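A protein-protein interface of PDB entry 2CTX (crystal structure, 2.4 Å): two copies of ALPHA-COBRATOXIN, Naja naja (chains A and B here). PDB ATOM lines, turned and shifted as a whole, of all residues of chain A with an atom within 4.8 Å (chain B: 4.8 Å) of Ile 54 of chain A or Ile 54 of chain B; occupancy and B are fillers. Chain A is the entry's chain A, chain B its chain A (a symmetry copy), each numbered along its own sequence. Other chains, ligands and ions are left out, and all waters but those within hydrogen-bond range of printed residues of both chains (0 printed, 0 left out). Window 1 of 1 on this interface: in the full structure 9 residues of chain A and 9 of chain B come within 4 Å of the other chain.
Cys 45 of chain A touches none of the printed residues of chain B.
Printed residues of chain B within 4 Å of Asp 53 of chain A: Gln 55 and Cys 56.
Of chain B, only Ile 54, Gln 55 and Cys 56 come within 4 Å of Ile 54 of chain A.
Of the printed residues of chain A, Asp 53 of chain B touches Gln 55 and Cys 56.
Ile 54 of chain B touches three residues of chain A.
Printed residues of chain A within 4 Å of Cys 56 of chain B: Asp 53 (3.7 Å) and Ile 54 (3.0 Å).
The nearest printed residue of chain A that does not touch Ile 54 of chain B is Cys 45 of chain A (4.8 Å).
Of the 11 printed residues of chain B, 4 touch a printed residue of chain A.
Printed residues of chain B that touch a printed residue of chain A: Asp 53, Ile 54, Gln 55 and Cys 56.
Of the 11 printed residues of chain A, 4 touch a printed residue of chain B.
Hydrophobic or aromatic side chains of chain A that line the printed part of chain B: Ile 54.
Among the printed residues, 9 pairs touch across the chains.
The side-chain carboxylate (OD1) of Asp 53 of chain A lies close to the side-chain amide oxygen (OE1) of Gln 55 of chain B (2.5 Å).
The backbone NH of Cys 56 of chain B lies within hydrogen-bond range of the backbone carbonyl oxygen of Ile 54 of chain A, at 3.0 Å.
The side-chain carboxylate (OD1) of Asp 53 of chain B lies close to the side-chain amide oxygen (OE1) of Gln 55 of chain A (2.5 Å).
O of Ile 54 of chain B lies within hydrogen-bond range of N of Cys 56 of chain A.
N of Gln 55 of chain A is in hydrogen-bond range of O of Thr 22 of chain A, at 2.7 Å.
SG of Cys 56 of chain A is disulfide-bonded to SG of Cys 45 of chain A (2.1 Å).
The backbone carbonyl oxygen (O) of Thr 22 of chain B lies within hydrogen-bond range of the backbone NH (N) of Gln 55 of chain B (2.7 Å).
SG of Cys 56 of chain B is disulfide-bonded to SG of Cys 45 of chain B (2.1 Å).
Cys 56 of chain B touches Asp 53 of chain A.
O of Ile 54 of chain A touches O of Ile 54 of chain B, at 3.9 Å.
Ile 54 of chain A touches Gln 55 of chain B.
Ile 54 of chain B touches Gln 55 of chain A (O to CA, 3.3 Å).
Asp 53 of chain B touches Cys 56 of chain A (CA to O, 3.7 Å).
Asp 53 of chain A touches Gln 55 of chain B, and with the chains exchanged Gln 55 of chain A touches Asp 53 of chain B.
Asp 53 of chain A touches Cys 56 of chain B, and with the chains exchanged Cys 56 of chain A touches Asp 53 of chain B.
Ile 54 of chain A touches Gln 55 of chain B, and with the chains exchanged Gln 55 of chain A touches Ile 54 of chain B.
Ile 54 of chain A touches Cys 56 of chain B, and with the chains exchanged Cys 56 of chain A touches Ile 54 of chain B.
Positions printed for both chains: 21, 22, 23, 45, 46, 48, 52, 53, 54, 55 and 56.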
ATOM      1  N   TYR A  21      15.568 -10.486  13.667  1.00  0.00           N
ATOM      2  CA  TYR A  21      15.026  -9.842  12.455  1.00  0.00           C
ATOM      3  C   TYR A  21      16.154  -9.487  11.478  1.00  0.00           C
ATOM      4  O   TYR A  21      17.361  -9.240  11.768  1.00  0.00           O
ATOM      5  CB  TYR A  21      14.010  -8.730  12.897  1.00  0.00           C
ATOM      6  CG  TYR A  21      14.750  -7.468  13.232  1.00  0.00           C
ATOM      7  CD1 TYR A  21      15.484  -6.825  12.241  1.00  0.00           C
ATOM      8  CD2 TYR A  21      14.751  -6.977  14.546  1.00  0.00           C
ATOM      9  CE1 TYR A  21      16.221  -5.682  12.510  1.00  0.00           C
ATOM     10  CE2 TYR A  21      15.458  -5.801  14.865  1.00  0.00           C
ATOM     11  CZ  TYR A  21      16.201  -5.198  13.834  1.00  0.00           C
ATOM     12  OH  TYR A  21      16.946  -4.043  14.073  1.00  0.00           O
ATOM     13  N   THR A  22      15.769  -9.517  10.212  1.00  0.00           N
ATOM     14  CA  THR A  22      16.490  -9.197   9.001  1.00  0.00           C
ATOM     15  C   THR A  22      15.564  -8.165   8.305  1.00  0.00           C
ATOM     16  O   THR A  22      14.351  -8.418   8.231  1.00  0.00           O
ATOM     17  CB  THR A  22      16.730 -10.322   7.987  1.00  0.00           C
ATOM     18  OG1 THR A  22      17.199 -11.460   8.706  1.00  0.00           O
ATOM     19  CG2 THR A  22      17.623  -9.909   6.819  1.00  0.00           C
ATOM     20  N   LYS A  23      16.106  -7.063   7.833  1.00  0.00           N
ATOM     21  CA  LYS A  23      15.342  -5.993   7.182  1.00  0.00           C
ATOM     22  C   LYS A  23      16.088  -5.789   5.848  1.00  0.00           C
ATOM     23  O   LYS A  23      17.246  -5.475   6.114  1.00  0.00           O
ATOM     24  CB  LYS A  23      15.535  -4.633   7.822  1.00  0.00           C
ATOM     25  CG  LYS A  23      14.399  -4.144   8.706  1.00  0.00           C
ATOM     26  CD  LYS A  23      14.886  -2.980   9.557  1.00  0.00           C
ATOM     27  CE  LYS A  23      14.570  -3.352  10.998  1.00  0.00           C
ATOM     28  NZ  LYS A  23      14.223  -2.030  11.639  1.00  0.00           N
ATOM     29  N   CYS A  45       8.254  -8.427  16.217  1.00  0.00           N
ATOM     30  CA  CYS A  45       8.546  -8.281  14.779  1.00  0.00           C
ATOM     31  C   CYS A  45       8.232  -6.834  14.413  1.00  0.00           C
ATOM     32  O   CYS A  45       7.072  -6.402  14.447  1.00  0.00           O
ATOM     33  CB  CYS A  45       7.703  -9.270  14.002  1.00  0.00           C
ATOM     34  SG  CYS A  45       8.353  -9.349  12.354  1.00  0.00           S
ATOM     35  N   PRO A  46       9.245  -6.065  14.088  1.00  0.00           N
ATOM     36  CA  PRO A  46       9.156  -4.654  13.751  1.00  0.00           C
ATOM     37  C   PRO A  46       8.369  -4.304  12.500  1.00  0.00           C
ATOM     38  O   PRO A  46       8.150  -5.121  11.605  1.00  0.00           O
ATOM     39  CB  PRO A  46      10.644  -4.289  13.637  1.00  0.00           C
ATOM     40  CG  PRO A  46      11.095  -5.533  12.892  1.00  0.00           C
ATOM     41  CD  PRO A  46      10.677  -6.556  13.964  1.00  0.00           C
ATOM     42  N   VAL A  48       7.261  -2.257   9.143  1.00  0.00           N
ATOM     43  CA  VAL A  48       7.925  -1.828   7.911  1.00  0.00           C
ATOM     44  C   VAL A  48       7.370  -0.603   7.219  1.00  0.00           C
ATOM     45  O   VAL A  48       6.167  -0.356   7.309  1.00  0.00           O
ATOM     46  CB  VAL A  48       8.042  -3.078   7.000  1.00  0.00           C
ATOM     47  CG1 VAL A  48       9.443  -3.647   7.145  1.00  0.00           C
ATOM     48  CG2 VAL A  48       6.905  -4.072   7.219  1.00  0.00           C
ATOM     49  N   VAL A  52      10.598  -1.702   2.291  1.00  0.00           N
ATOM     50  CA  VAL A  52      11.651  -2.357   3.096  1.00  0.00           C
ATOM     51  C   VAL A  52      11.075  -3.735   3.381  1.00  0.00           C
ATOM     52  O   VAL A  52       9.846  -3.822   3.454  1.00  0.00           O
ATOM     53  CB  VAL A  52      11.753  -1.502   4.380  1.00  0.00           C
ATOM     54  CG1 VAL A  52      12.163  -2.347   5.578  1.00  0.00           C
ATOM     55  CG2 VAL A  52      12.598  -0.278   4.182  1.00  0.00           C
ATOM     56  N   ASP A  53      11.888  -4.742   3.561  1.00  0.00           N
ATOM     57  CA  ASP A  53      11.171  -6.036   3.792  1.00  0.00           C
ATOM     58  C   ASP A  53      11.711  -6.646   5.021  1.00  0.00           C
ATOM     59  O   ASP A  53      12.863  -6.328   5.295  1.00  0.00           O
ATOM     60  CB  ASP A  53      10.768  -6.490   2.448  1.00  0.00           C
ATOM     61  CG  ASP A  53      11.086  -7.927   2.187  1.00  0.00           C
ATOM     62  OD1 ASP A  53      11.275  -8.633   3.156  1.00  0.00           O
ATOM     63  OD2 ASP A  53      11.103  -8.048   0.873  1.00  0.00           O
ATOM     64  N   ILE A  54      10.932  -7.317   5.806  1.00  0.00           N
ATOM     65  CA  ILE A  54      11.352  -7.835   7.103  1.00  0.00           C
ATOM     66  C   ILE A  54      11.149  -9.303   7.281  1.00  0.00           C
ATOM     67  O   ILE A  54      10.178  -9.903   6.798  1.00  0.00           O
ATOM     68  CB  ILE A  54      10.631  -6.952   8.158  1.00  0.00           C
ATOM     69  CG1 ILE A  54      10.970  -7.240   9.614  1.00  0.00           C
ATOM     70  CG2 ILE A  54       9.128  -6.752   8.059  1.00  0.00           C
ATOM     71  CD1 ILE A  54      12.217  -6.437   9.992  1.00  0.00           C
ATOM     72  N   GLN A  55      12.076  -9.932   7.982  1.00  0.00           N
ATOM     73  CA  GLN A  55      12.023 -11.354   8.313  1.00  0.00           C
ATOM     74  C   GLN A  55      12.302 -11.468   9.811  1.00  0.00           C
ATOM     75  O   GLN A  55      13.239 -10.889  10.352  1.00  0.00           O
ATOM     76  CB  GLN A  55      12.892 -12.305   7.538  1.00  0.00           C
ATOM     77  CG  GLN A  55      12.930 -13.684   8.151  1.00  0.00           C
ATOM     78  CD  GLN A  55      13.377 -14.854   7.302  1.00  0.00           C
ATOM     79  OE1 GLN A  55      12.869 -16.012   7.366  1.00  0.00           O
ATOM     80  NE2 GLN A  55      14.377 -14.688   6.418  1.00  0.00           N
ATOM     81  N   CYS A  56      11.383 -12.169  10.421  1.00  0.00           N
ATOM     82  CA  CYS A  56      11.374 -12.459  11.835  1.00  0.00           C
ATOM     83  C   CYS A  56      11.251 -13.940  12.184  1.00  0.00           C
ATOM     84  O   CYS A  56      10.310 -14.576  11.710  1.00  0.00           O
ATOM     85  CB  CYS A  56      10.246 -11.759  12.556  1.00  0.00           C
ATOM     86  SG  CYS A  56      10.303  -9.996  12.553  1.00  0.00           S
ATOM     87  N   TYR B  21       2.591 -11.649   3.170  1.00  0.00           N
ATOM     88  CA  TYR B  21       3.353 -12.471   4.129  1.00  0.00           C
ATOM     89  C   TYR B  21       3.546 -13.895   3.592  1.00  0.00           C
ATOM     90  O   TYR B  21       2.794 -14.509   2.780  1.00  0.00           O
ATOM     91  CB  TYR B  21       2.737 -12.263   5.559  1.00  0.00           C
ATOM     92  CG  TYR B  21       1.549 -13.162   5.737  1.00  0.00           C
ATOM     93  CD1 TYR B  21       1.725 -14.540   5.685  1.00  0.00           C
ATOM     94  CD2 TYR B  21       0.266 -12.616   5.893  1.00  0.00           C
ATOM     95  CE1 TYR B  21       0.654 -15.413   5.799  1.00  0.00           C
ATOM     96  CE2 TYR B  21      -0.852 -13.460   6.045  1.00  0.00           C
ATOM     97  CZ  TYR B  21      -0.627 -14.845   5.966  1.00  0.00           C
ATOM     98  OH  TYR B  21      -1.683 -15.748   6.085  1.00  0.00           O
ATOM     99  N   THR B  22       4.666 -14.459   4.015  1.00  0.00           N
ATOM    100  CA  THR B  22       5.192 -15.787   3.797  1.00  0.00           C
ATOM    101  C   THR B  22       5.469 -16.295   5.236  1.00  0.00           C
ATOM    102  O   THR B  22       6.059 -15.539   6.024  1.00  0.00           O
ATOM    103  CB  THR B  22       6.509 -15.922   3.024  1.00  0.00           C
ATOM    104  OG1 THR B  22       6.421 -15.092   1.869  1.00  0.00           O
ATOM    105  CG2 THR B  22       6.894 -17.369   2.727  1.00  0.00           C
ATOM    106  N   LYS B  23       5.056 -17.500   5.560  1.00  0.00           N
ATOM    107  CA  LYS B  23       5.225 -18.089   6.893  1.00  0.00           C
ATOM    108  C   LYS B  23       5.900 -19.444   6.598  1.00  0.00           C
ATOM    109  O   LYS B  23       5.147 -20.084   5.869  1.00  0.00           O
ATOM    110  CB  LYS B  23       3.927 -18.555   7.520  1.00  0.00           C
ATOM    111  CG  LYS B  23       3.348 -17.657   8.603  1.00  0.00           C
ATOM    112  CD  LYS B  23       1.897 -18.042   8.857  1.00  0.00           C
ATOM    113  CE  LYS B  23       1.090 -16.761   8.703  1.00  0.00           C
ATOM    114  NZ  LYS B  23      -0.011 -16.911   9.724  1.00  0.00           N
ATOM    115  N   CYS B  45       1.887  -7.220   9.814  1.00  0.00           N
ATOM    116  CA  CYS B  45       2.824  -8.360   9.843  1.00  0.00           C
ATOM    117  C   CYS B  45       2.420  -9.227  11.032  1.00  0.00           C
ATOM    118  O   CYS B  45       2.536  -8.815  12.194  1.00  0.00           O
ATOM    119  CB  CYS B  45       4.238  -7.833   9.966  1.00  0.00           C
ATOM    120  SG  CYS B  45       5.340  -9.173   9.603  1.00  0.00           S
ATOM    121  N   PRO B  46       1.920 -10.411  10.768  1.00  0.00           N
ATOM    122  CA  PRO B  46       1.441 -11.363  11.756  1.00  0.00           C
ATOM    123  C   PRO B  46       2.474 -11.913  12.726  1.00  0.00           C
ATOM    124  O   PRO B  46       3.681 -11.894  12.487  1.00  0.00           O
ATOM    125  CB  PRO B  46       0.845 -12.449  10.848  1.00  0.00           C
ATOM    126  CG  PRO B  46       1.951 -12.465   9.808  1.00  0.00           C
ATOM    127  CD  PRO B  46       1.817 -10.995   9.369  1.00  0.00           C
ATOM    128  N   VAL B  48       4.313 -14.550  15.245  1.00  0.00           N
ATOM    129  CA  VAL B  48       4.814 -15.921  15.141  1.00  0.00           C
ATOM    130  C   VAL B  48       4.862 -16.736  16.414  1.00  0.00           C
ATOM    131  O   VAL B  48       5.050 -16.163  17.488  1.00  0.00           O
ATOM    132  CB  VAL B  48       6.160 -15.855  14.375  1.00  0.00           C
ATOM    133  CG1 VAL B  48       5.901 -16.210  12.920  1.00  0.00           C
ATOM    134  CG2 VAL B  48       6.904 -14.544  14.605  1.00  0.00           C
ATOM    135  N   VAL B  52       8.213 -20.960  13.798  1.00  0.00           N
ATOM    136  CA  VAL B  52       7.604 -20.665  12.484  1.00  0.00           C
ATOM    137  C   VAL B  52       8.323 -19.402  12.035  1.00  0.00           C
ATOM    138  O   VAL B  52       8.715 -18.637  12.922  1.00  0.00           O
ATOM    139  CB  VAL B  52       6.114 -20.396  12.792  1.00  0.00           C
ATOM    140  CG1 VAL B  52       5.515 -19.398  11.811  1.00  0.00           C
ATOM    141  CG2 VAL B  52       5.323 -21.664  12.926  1.00  0.00           C
ATOM    142  N   ASP B  53       8.467 -19.169  10.757  1.00  0.00           N
ATOM    143  CA  ASP B  53       9.228 -17.910  10.476  1.00  0.00           C
ATOM    144  C   ASP B  53       8.435 -17.096   9.537  1.00  0.00           C
ATOM    145  O   ASP B  53       7.674 -17.730   8.814  1.00  0.00           O
ATOM    146  CB  ASP B  53      10.645 -18.277  10.657  1.00  0.00           C
ATOM    147  CG  ASP B  53      11.526 -17.810   9.544  1.00  0.00           C
ATOM    148  OD1 ASP B  53      11.100 -16.913   8.846  1.00  0.00           O
ATOM    149  OD2 ASP B  53      12.601 -18.573   9.605  1.00  0.00           O
ATOM    150  N   ILE B  54       8.449 -15.805   9.630  1.00  0.00           N
ATOM    151  CA  ILE B  54       7.592 -14.934   8.833  1.00  0.00           C
ATOM    152  C   ILE B  54       8.321 -13.892   8.052  1.00  0.00           C
ATOM    153  O   ILE B  54       9.337 -13.330   8.483  1.00  0.00           O
ATOM    154  CB  ILE B  54       6.532 -14.376   9.822  1.00  0.00           C
ATOM    155  CG1 ILE B  54       5.454 -13.490   9.212  1.00  0.00           C
ATOM    156  CG2 ILE B  54       6.989 -13.731  11.118  1.00  0.00           C
ATOM    157  CD1 ILE B  54       4.317 -14.383   8.708  1.00  0.00           C
ATOM    158  N   GLN B  55       7.820 -13.608   6.863  1.00  0.00           N
ATOM    159  CA  GLN B  55       8.356 -12.576   5.978  1.00  0.00           C
ATOM    160  C   GLN B  55       7.171 -11.729   5.519  1.00  0.00           C
ATOM    161  O   GLN B  55       6.131 -12.226   5.096  1.00  0.00           O
ATOM    162  CB  GLN B  55       9.190 -13.003   4.802  1.00  0.00           C
ATOM    163  CG  GLN B  55       9.455 -11.870   3.840  1.00  0.00           C
ATOM    164  CD  GLN B  55      10.602 -11.989   2.862  1.00  0.00           C
ATOM    165  OE1 GLN B  55      11.350 -11.025   2.522  1.00  0.00           O
ATOM    166  NE2 GLN B  55      10.868 -13.179   2.294  1.00  0.00           N
ATOM    167  N   CYS B  56       7.381 -10.455   5.722  1.00  0.00           N
ATOM    168  CA  CYS B  56       6.450  -9.405   5.386  1.00  0.00           C
ATOM    169  C   CYS B  56       7.028  -8.292   4.516  1.00  0.00           C
ATOM    170  O   CYS B  56       8.047  -7.719   4.899  1.00  0.00           O
ATOM    171  CB  CYS B  56       5.879  -8.731   6.612  1.00  0.00           C
ATOM    172  SG  CYS B  56       4.903  -9.750   7.670  1.00  0.00           S
